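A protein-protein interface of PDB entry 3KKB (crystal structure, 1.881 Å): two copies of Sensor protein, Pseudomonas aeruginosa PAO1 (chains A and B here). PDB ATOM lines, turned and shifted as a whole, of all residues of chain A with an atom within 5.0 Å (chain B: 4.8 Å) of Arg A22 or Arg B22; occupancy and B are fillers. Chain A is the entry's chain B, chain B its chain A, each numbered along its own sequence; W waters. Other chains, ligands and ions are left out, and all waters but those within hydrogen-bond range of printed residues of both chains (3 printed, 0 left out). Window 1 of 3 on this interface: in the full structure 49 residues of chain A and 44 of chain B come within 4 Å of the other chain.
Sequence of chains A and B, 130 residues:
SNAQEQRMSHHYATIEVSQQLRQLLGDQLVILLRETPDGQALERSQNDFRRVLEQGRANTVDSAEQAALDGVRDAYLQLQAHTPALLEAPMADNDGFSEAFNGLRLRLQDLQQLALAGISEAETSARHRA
NE2 of Gln B112 lies within hydrogen-bond range of OG of Ser A18 (3.1 Å). The side-chain amide oxygen (OE1) of Gln A19 sits at hydrogen-bond distance from the guanidinium group (NH1) of Arg B22, 2.9 Å away. The side-chain amide oxygen (OE1) of Gln A112 sits at hydrogen-bond distance from the guanidinium group (NH1) of Arg B22 (2.8 Å). The guanidinium group (NH1) of Arg A22 sits close to the side-chain amide nitrogen (NE2) of Gln B19. The side-chain amide nitrogen of Gln B112 lies within hydrogen-bond range of the side-chain amide oxygen of Gln A19. OE1 of Gln B112 sits at hydrogen-bond distance from NE2 of Gln A112, 3.1 Å away. NE2 of Gln B19 sits at hydrogen-bond distance from OE1 of Gln A112, at 2.7 Å. OE1 of Gln B112 lies within hydrogen-bond range of NH1 of Arg A22 (2.8 Å).
OE1 of Gln B112 lies within hydrogen-bond range of NE2 of Gln B19, at 3.0 Å. The side-chain amide nitrogen of Gln A112 sits at hydrogen-bond distance from the side-chain amide oxygen of Gln A19. O of Gln A23 lies within hydrogen-bond range of NH2 of Arg A105.
Leu B108 touches Leu A21. Arg B22 touches Arg A22 (CB to NH2, 3.5 Å). Arg A22 touches Leu B108 (CG to CB, 3.8 Å). NH2 of Arg A22 touches CG of Gln B109, at 3.5 Å. CB of Arg A105 touches CD2 of Leu B25, 3.98 Å away. Leu B21 touches Leu A108. Leu A108 touches Arg B22. Leu B25 touches Leu A108. CB of Gln A112 touches OG of Ser B18, at 3.3 Å.
Arg A22 touches just these residues of chain B: Gln B19 (3.5 Å), Arg B22 (3.5 Å), Leu B108 (3.8 Å), Gln B109 (3.5 Å) and Gln B112 (2.8 Å). Of chain A, only Gln A19 (2.9 Å), Arg A22 (3.5 Å), Leu A108 (3.7 Å) and Gln A112 (2.8 Å) come within 4 Å of Arg B22. Printed residues of chain A within 4 Å of Ser B18: Gln A112. Printed residues of chain B within 4 Å of Leu A21: Leu B108. Of the printed residues of chain B, Arg A105 touches Leu B25 (3.98 Å). Of the printed residues of chain B, Ser A18 touches Gln B112. Of the printed residues of chain B, Gln A112 touches Ser B18 (3.3 Å), Gln B19 (2.7 Å), Arg B22 (2.8 Å) and Gln B112 (3.1 Å). Gly B26 touches none of the printed residues of chain A. The nearest printed residue of chain B that does not touch Leu A108 is Ser B18 (4.4 Å).
Of the 12 printed residues of chain B, 8 touch a printed residue of chain A. Along chain B the printed residues that touch a printed residue of chain A span positions 18 to 112. Of the 13 printed residues of chain A, 7 touch a printed residue of chain B. Printed residues of chain A that touch a printed residue of chain B: Ser A18, Gln A19, Leu A21, Arg A22, Arg A105, Leu A108 and Gln A112. Hydrophobic or aromatic side chains of chain A that line the printed part of chain B: Leu A21 and Leu A108.
Ser A18 touches Gln B112, and with the chains exchanged Gln A112 touches Ser B18. Gln A19 touches Arg B22, and with the chains exchanged Arg A22 touches Gln B19. Gln A19 touches Gln B112, and with the chains exchanged Gln A112 touches Gln B19. Leu A21 touches Leu B108, and with the chains exchanged Leu A108 touches Leu B21. Of the 17 pairs that touch across the chains among the printed residues, 14 have their exchanged pair printed and touching as well.
Water W1 lies within hydrogen-bond range of the side-chain amide oxygen (OE1) of Gln B109 and the guanidinium group (NH2) of Arg A22. Water W2 lies within hydrogen-bond range of the backbone carbonyl oxygen (O) of Gln A19 (2.8 Å), the guanidinium group (NH2) of Arg B22 (2.9 Å), the side-chain amide oxygen (OE1) of Gln A109 (3.0 Å) and the backbone NH (N) of Gln A23 (3.4 Å). Water W3 bridges the backbone carbonyl oxygen (O) of Gln B19 and the guanidinium group (NH2) of Arg A22.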
ATOM      1  N   SER A  18      23.077  28.692   9.723  1.00  0.00           N
ATOM      2  CA  SER A  18      23.700  27.417  10.037  1.00  0.00           C
ATOM      3  C   SER A  18      22.779  26.265   9.652  1.00  0.00           C
ATOM      4  O   SER A  18      23.257  25.228   9.227  1.00  0.00           O
ATOM      5  CB  SER A  18      24.093  27.309  11.509  1.00  0.00           C
ATOM      6  OG  SER A  18      22.956  27.412  12.358  1.00  0.00           O
ATOM      7  N   GLN A  19      21.471  26.444   9.799  1.00  0.00           N
ATOM      8  CA  GLN A  19      20.511  25.412   9.372  1.00  0.00           C
ATOM      9  C   GLN A  19      20.570  25.181   7.851  1.00  0.00           C
ATOM     10  O   GLN A  19      20.503  24.034   7.383  1.00  0.00           O
ATOM     11  CB  GLN A  19      19.088  25.778   9.809  1.00  0.00           C
ATOM     12  CG  GLN A  19      18.026  24.704   9.541  1.00  0.00           C
ATOM     13  CD  GLN A  19      18.064  23.574  10.575  1.00  0.00           C
ATOM     14  OE1 GLN A  19      19.040  23.422  11.312  1.00  0.00           O
ATOM     15  NE2 GLN A  19      16.995  22.778  10.626  1.00  0.00           N
ATOM     16  N   GLN A  20      20.710  26.262   7.081  1.00  0.00           N
ATOM     17  CA  GLN A  20      20.825  26.142   5.622  1.00  0.00           C
ATOM     18  C   GLN A  20      22.064  25.347   5.267  1.00  0.00           C
ATOM     19  O   GLN A  20      21.997  24.423   4.456  1.00  0.00           O
ATOM     20  CB  GLN A  20      20.900  27.512   4.933  1.00  0.00           C
ATOM     21  CG  GLN A  20      19.628  28.362   5.055  1.00  0.00           C
ATOM     22  CD  GLN A  20      19.834  29.737   4.466  1.00  0.00           C
ATOM     23  OE1 GLN A  20      20.470  30.589   5.081  1.00  0.00           O
ATOM     24  NE2 GLN A  20      19.313  29.957   3.268  1.00  0.00           N
ATOM     25  N   LEU A  21      23.196  25.716   5.866  1.00  0.00           N
ATOM     26  CA  LEU A  21      24.455  25.008   5.603  1.00  0.00           C
ATOM     27  C   LEU A  21      24.377  23.536   6.013  1.00  0.00           C
ATOM     28  O   LEU A  21      24.887  22.663   5.307  1.00  0.00           O
ATOM     29  CB  LEU A  21      25.634  25.700   6.294  1.00  0.00           C
ATOM     30  CG  LEU A  21      25.933  27.112   5.768  1.00  0.00           C
ATOM     31  CD1 LEU A  21      26.966  27.807   6.648  1.00  0.00           C
ATOM     32  CD2 LEU A  21      26.376  27.103   4.301  1.00  0.00           C
ATOM     33  N   ARG A  22      23.748  23.247   7.151  1.00  0.00           N
ATOM     34  CA  ARG A  22      23.563  21.851   7.551  1.00  0.00           C
ATOM     35  C   ARG A  22      22.755  21.062   6.521  1.00  0.00           C
ATOM     36  O   ARG A  22      23.095  19.920   6.201  1.00  0.00           O
ATOM     37  CB  ARG A  22      22.915  21.734   8.939  1.00  0.00           C
ATOM     38  CG  ARG A  22      23.859  22.128  10.064  1.00  0.00           C
ATOM     39  CD  ARG A  22      23.254  21.871  11.451  1.00  0.00           C
ATOM     40  NE  ARG A  22      23.449  20.479  11.839  1.00  0.00           N
ATOM     41  CZ  ARG A  22      23.115  19.982  13.024  1.00  0.00           C
ATOM     42  NH1 ARG A  22      22.575  20.771  13.944  1.00  0.00           N
ATOM     43  NH2 ARG A  22      23.355  18.709  13.298  1.00  0.00           N
ATOM     44  N   GLN A  23      21.683  21.655   6.012  1.00  0.00           N
ATOM     45  CA  GLN A  23      20.893  20.972   4.990  1.00  0.00           C
ATOM     46  C   GLN A  23      21.687  20.766   3.711  1.00  0.00           C
ATOM     47  O   GLN A  23      21.593  19.712   3.080  1.00  0.00           O
ATOM     48  CB  GLN A  23      19.604  21.721   4.650  1.00  0.00           C
ATOM     49  CG  GLN A  23      18.760  20.936   3.633  1.00  0.00           C
ATOM     50  CD  GLN A  23      17.650  21.749   3.017  1.00  0.00           C
ATOM     51  OE1 GLN A  23      16.838  22.359   3.722  1.00  0.00           O
ATOM     52  NE2 GLN A  23      17.609  21.771   1.692  1.00  0.00           N
ATOM     53  N   LEU A  24      22.468  21.770   3.327  1.00  0.00           N
ATOM     54  CA  LEU A  24      23.188  21.705   2.062  1.00  0.00           C
ATOM     55  C   LEU A  24      24.313  20.674   2.139  1.00  0.00           C
ATOM     56  O   LEU A  24      24.580  19.949   1.174  1.00  0.00           O
ATOM     57  CB  LEU A  24      23.679  23.102   1.654  1.00  0.00           C
ATOM     58  CG  LEU A  24      22.512  24.054   1.336  1.00  0.00           C
ATOM     59  CD1 LEU A  24      22.960  25.519   1.172  1.00  0.00           C
ATOM     60  CD2 LEU A  24      21.733  23.594   0.106  1.00  0.00           C
ATOM     61  N   LEU A  25      24.935  20.576   3.306  1.00  0.00           N
ATOM     62  CA  LEU A  25      25.923  19.526   3.546  1.00  0.00           C
ATOM     63  C   LEU A  25      25.280  18.134   3.440  1.00  0.00           C
ATOM     64  O   LEU A  25      25.841  17.216   2.828  1.00  0.00           O
ATOM     65  CB  LEU A  25      26.605  19.722   4.911  1.00  0.00           C
ATOM     66  CG  LEU A  25      27.655  18.666   5.296  1.00  0.00           C
ATOM     67  CD1 LEU A  25      28.698  18.509   4.206  1.00  0.00           C
ATOM     68  CD2 LEU A  25      28.321  18.962   6.649  1.00  0.00           C
ATOM     69  N   GLY A  26      24.102  17.977   4.031  1.00  0.00           N
ATOM     70  CA  GLY A  26      23.389  16.712   3.964  1.00  0.00           C
ATOM     71  C   GLY A  26      22.979  16.382   2.538  1.00  0.00           C
ATOM     72  O   GLY A  26      23.029  15.219   2.137  1.00  0.00           O
ATOM     73  N   ARG A 105      17.108  12.182   7.892  1.00  0.00           N
ATOM     74  CA  ARG A 105      17.769  13.450   8.200  1.00  0.00           C
ATOM     75  C   ARG A 105      16.860  14.641   7.927  1.00  0.00           C
ATOM     76  O   ARG A 105      16.952  15.651   8.607  1.00  0.00           O
ATOM     77  CB  ARG A 105      19.101  13.586   7.462  1.00  0.00           C
ATOM     78  CG  ARG A 105      18.961  13.702   5.964  1.00  0.00           C
ATOM     79  CD  ARG A 105      19.187  15.123   5.526  1.00  0.00           C
ATOM     80  NE  ARG A 105      18.989  15.248   4.092  1.00  0.00           N
ATOM     81  CZ  ARG A 105      19.349  16.308   3.382  1.00  0.00           C
ATOM     82  NH1 ARG A 105      19.119  16.331   2.083  1.00  0.00           N
ATOM     83  NH2 ARG A 105      19.929  17.343   3.976  1.00  0.00           N
ATOM     84  N   LEU A 108      14.479  14.841  10.961  1.00  0.00           N
ATOM     85  CA  LEU A 108      15.136  15.458  12.112  1.00  0.00           C
ATOM     86  C   LEU A 108      15.249  16.966  11.933  1.00  0.00           C
ATOM     87  O   LEU A 108      15.034  17.742  12.875  1.00  0.00           O
ATOM     88  CB  LEU A 108      16.538  14.873  12.337  1.00  0.00           C
ATOM     89  CG  LEU A 108      16.626  13.466  12.927  1.00  0.00           C
ATOM     90  CD1 LEU A 108      18.079  13.016  13.046  1.00  0.00           C
ATOM     91  CD2 LEU A 108      15.921  13.401  14.285  1.00  0.00           C
ATOM     92  N   GLN A 109      15.602  17.376  10.720  1.00  0.00           N
ATOM     93  CA  GLN A 109      15.656  18.798  10.396  1.00  0.00           C
ATOM     94  C   GLN A 109      14.305  19.475  10.606  1.00  0.00           C
ATOM     95  O   GLN A 109      14.229  20.558  11.182  1.00  0.00           O
ATOM     96  CB  GLN A 109      16.129  19.005   8.947  1.00  0.00           C
ATOM     97  CG  GLN A 109      15.881  20.409   8.448  1.00  0.00           C
ATOM     98  CD  GLN A 109      16.393  20.627   7.043  1.00  0.00           C
ATOM     99  OE1 GLN A 109      17.511  20.243   6.713  1.00  0.00           O
ATOM    100  NE2 GLN A 109      15.577  21.256   6.207  1.00  0.00           N
ATOM    101  N   GLN A 112      13.384  19.767  14.364  1.00  0.00           N
ATOM    102  CA  GLN A 112      14.057  20.914  14.959  1.00  0.00           C
ATOM    103  C   GLN A 112      13.379  22.247  14.568  1.00  0.00           C
ATOM    104  O   GLN A 112      13.195  23.125  15.405  1.00  0.00           O
ATOM    105  CB  GLN A 112      15.542  20.961  14.591  1.00  0.00           C
ATOM    106  CG  GLN A 112      16.269  22.140  15.253  1.00  0.00           C
ATOM    107  CD  GLN A 112      17.746  22.207  14.903  1.00  0.00           C
ATOM    108  OE1 GLN A 112      18.491  21.257  15.145  1.00  0.00           O
ATOM    109  NE2 GLN A 112      18.179  23.347  14.336  1.00  0.00           N
ATOM    110  N   SER B  18      16.005  17.090  19.438  1.00  0.00           N
ATOM    111  CA  SER B  18      16.333  17.150  18.016  1.00  0.00           C
ATOM    112  C   SER B  18      17.827  17.377  17.784  1.00  0.00           C
ATOM    113  O   SER B  18      18.432  16.742  16.919  1.00  0.00           O
ATOM    114  CB  SER B  18      15.479  18.197  17.270  1.00  0.00           C
ATOM    115  OG  SER B  18      15.873  19.531  17.583  1.00  0.00           O
ATOM    116  N   GLN B  19      18.422  18.283  18.546  1.00  0.00           N
ATOM    117  CA  GLN B  19      19.850  18.552  18.393  1.00  0.00           C
ATOM    118  C   GLN B  19      20.683  17.310  18.739  1.00  0.00           C
ATOM    119  O   GLN B  19      21.640  16.979  18.036  1.00  0.00           O
ATOM    120  CB  GLN B  19      20.265  19.732  19.265  1.00  0.00           C
ATOM    121  CG  GLN B  19      19.807  21.097  18.730  1.00  0.00           C
ATOM    122  CD  GLN B  19      20.894  21.766  17.903  1.00  0.00           C
ATOM    123  OE1 GLN B  19      21.941  22.150  18.432  1.00  0.00           O
ATOM    124  NE2 GLN B  19      20.661  21.893  16.608  1.00  0.00           N
ATOM    125  N   GLN B  20      20.315  16.617  19.812  1.00  0.00           N
ATOM    126  CA  GLN B  20      21.041  15.396  20.199  1.00  0.00           C
ATOM    127  C   GLN B  20      20.903  14.282  19.179  1.00  0.00           C
ATOM    128  O   GLN B  20      21.883  13.612  18.863  1.00  0.00           O
ATOM    129  CB  GLN B  20      20.597  14.889  21.573  1.00  0.00           C
ATOM    130  CG  GLN B  20      21.009  15.758  22.726  1.00  0.00           C
ATOM    131  CD  GLN B  20      20.609  15.154  24.063  1.00  0.00           C
ATOM    132  OE1 GLN B  20      20.051  15.838  24.921  1.00  0.00           O
ATOM    133  NE2 GLN B  20      20.884  13.862  24.240  1.00  0.00           N
ATOM    134  N   LEU B  21      19.694  14.080  18.652  1.00  0.00           N
ATOM    135  CA  LEU B  21      19.494  13.067  17.616  1.00  0.00           C
ATOM    136  C   LEU B  21      20.307  13.389  16.365  1.00  0.00           C
ATOM    137  O   LEU B  21      20.898  12.507  15.749  1.00  0.00           O
ATOM    138  CB  LEU B  21      18.010  12.928  17.266  1.00  0.00           C
ATOM    139  CG  LEU B  21      17.133  12.396  18.412  1.00  0.00           C
ATOM    140  CD1 LEU B  21      15.697  12.240  17.926  1.00  0.00           C
ATOM    141  CD2 LEU B  21      17.678  11.070  18.940  1.00  0.00           C
ATOM    142  N   ARG B  22      20.363  14.662  15.997  1.00  0.00           N
ATOM    143  CA  ARG B  22      21.162  15.031  14.821  1.00  0.00           C
ATOM    144  C   ARG B  22      22.660  14.798  15.054  1.00  0.00           C
ATOM    145  O   ARG B  22      23.363  14.333  14.160  1.00  0.00           O
ATOM    146  CB  ARG B  22      20.870  16.468  14.421  1.00  0.00           C
ATOM    147  CG  ARG B  22      19.442  16.653  13.902  1.00  0.00           C
ATOM    148  CD  ARG B  22      19.160  18.131  13.597  1.00  0.00           C
ATOM    149  NE  ARG B  22      19.728  18.520  12.312  1.00  0.00           N
ATOM    150  CZ  ARG B  22      19.654  19.744  11.797  1.00  0.00           C
ATOM    151  NH1 ARG B  22      19.059  20.712  12.471  1.00  0.00           N
ATOM    152  NH2 ARG B  22      20.174  19.993  10.605  1.00  0.00           N
ATOM    153  N   GLN B  23      23.130  15.086  16.263  1.00  0.00           N
ATOM    154  CA  GLN B  23      24.524  14.806  16.640  1.00  0.00           C
ATOM    155  C   GLN B  23      24.852  13.313  16.532  1.00  0.00           C
ATOM    156  O   GLN B  23      25.878  12.929  15.974  1.00  0.00           O
ATOM    157  CB  GLN B  23      24.801  15.293  18.061  1.00  0.00           C
ATOM    158  CG  GLN B  23      24.815  16.817  18.210  1.00  0.00           C
ATOM    159  CD  GLN B  23      24.570  17.270  19.641  1.00  0.00           C
ATOM    160  OE1 GLN B  23      24.567  16.456  20.570  1.00  0.00           O
ATOM    161  NE2 GLN B  23      24.344  18.577  19.826  1.00  0.00           N
ATOM    162  N   LEU B  24      23.964  12.478  17.052  1.00  0.00           N
ATOM    163  CA  LEU B  24      24.146  11.025  17.014  1.00  0.00           C
ATOM    164  C   LEU B  24      24.089  10.447  15.600  1.00  0.00           C
ATOM    165  O   LEU B  24      24.855   9.543  15.262  1.00  0.00           O
ATOM    166  CB  LEU B  24      23.100  10.347  17.912  1.00  0.00           C
ATOM    167  CG  LEU B  24      23.294  10.651  19.406  1.00  0.00           C
ATOM    168  CD1 LEU B  24      22.112  10.173  20.244  1.00  0.00           C
ATOM    169  CD2 LEU B  24      24.582  10.000  19.884  1.00  0.00           C
ATOM    170  N   LEU B  25      23.180  10.954  14.777  1.00  0.00           N
ATOM    171  CA  LEU B  25      23.128  10.526  13.388  1.00  0.00           C
ATOM    172  C   LEU B  25      24.423  10.930  12.685  1.00  0.00           C
ATOM    173  O   LEU B  25      24.969  10.171  11.896  1.00  0.00           O
ATOM    174  CB  LEU B  25      21.920  11.121  12.667  1.00  0.00           C
ATOM    175  CG  LEU B  25      21.812  10.806  11.168  1.00  0.00           C
ATOM    176  CD1 LEU B  25      21.705   9.311  10.921  1.00  0.00           C
ATOM    177  CD2 LEU B  25      20.639  11.557  10.517  1.00  0.00           C
ATOM    178  N   GLY B  26      24.913  12.130  12.972  1.00  0.00           N
ATOM    179  CA  GLY B  26      26.203  12.555  12.448  1.00  0.00           C
ATOM    180  C   GLY B  26      27.326  11.614  12.856  1.00  0.00           C
ATOM    181  O   GLY B  26      28.138  11.234  12.012  1.00  0.00           O
ATOM    182  N   LEU B 108      29.485  23.109  12.312  1.00  0.00           N
ATOM    183  CA  LEU B 108      28.095  23.511  12.109  1.00  0.00           C
ATOM    184  C   LEU B 108      27.218  23.238  13.349  1.00  0.00           C
ATOM    185  O   LEU B 108      26.329  24.042  13.668  1.00  0.00           O
ATOM    186  CB  LEU B 108      27.511  22.830  10.877  1.00  0.00           C
ATOM    187  CG  LEU B 108      28.154  23.302   9.565  1.00  0.00           C
ATOM    188  CD1 LEU B 108      27.578  22.521   8.406  1.00  0.00           C
ATOM    189  CD2 LEU B 108      27.974  24.808   9.365  1.00  0.00           C
ATOM    190  N   GLN B 109      27.451  22.107  14.016  1.00  0.00           N
ATOM    191  CA  GLN B 109      26.722  21.760  15.247  1.00  0.00           C
ATOM    192  C   GLN B 109      27.009  22.791  16.326  1.00  0.00           C
ATOM    193  O   GLN B 109      26.098  23.279  16.987  1.00  0.00           O
ATOM    194  CB  GLN B 109      27.070  20.347  15.743  1.00  0.00           C
ATOM    195  CG  GLN B 109      26.464  19.220  14.897  1.00  0.00           C
ATOM    196  CD  GLN B 109      26.982  17.826  15.238  1.00  0.00           C
ATOM    197  OE1 GLN B 109      26.636  16.851  14.565  1.00  0.00           O
ATOM    198  NE2 GLN B 109      27.812  17.721  16.283  1.00  0.00           N
ATOM    199  N   GLN B 112      25.156  26.113  15.857  1.00  0.00           N
ATOM    200  CA  GLN B 112      23.766  26.020  16.281  1.00  0.00           C
ATOM    201  C   GLN B 112      23.627  25.966  17.793  1.00  0.00           C
ATOM    202  O   GLN B 112      22.716  26.580  18.351  1.00  0.00           O
ATOM    203  CB  GLN B 112      23.060  24.814  15.644  1.00  0.00           C
ATOM    204  CG  GLN B 112      22.959  24.913  14.149  1.00  0.00           C
ATOM    205  CD  GLN B 112      21.673  24.317  13.606  1.00  0.00           C
ATOM    206  OE1 GLN B 112      21.267  23.219  13.999  1.00  0.00           O
ATOM    207  NE2 GLN B 112      21.030  25.040  12.685  1.00  0.00           N
HETATM  208  O   HOH W   1      25.669  16.868  11.970  1.00  0.00           O
HETATM  209  O   HOH W   2      19.378  21.711   8.471  1.00  0.00           O
HETATM  210  O   HOH W   3      22.840  18.819  16.242  1.00  0.00           O
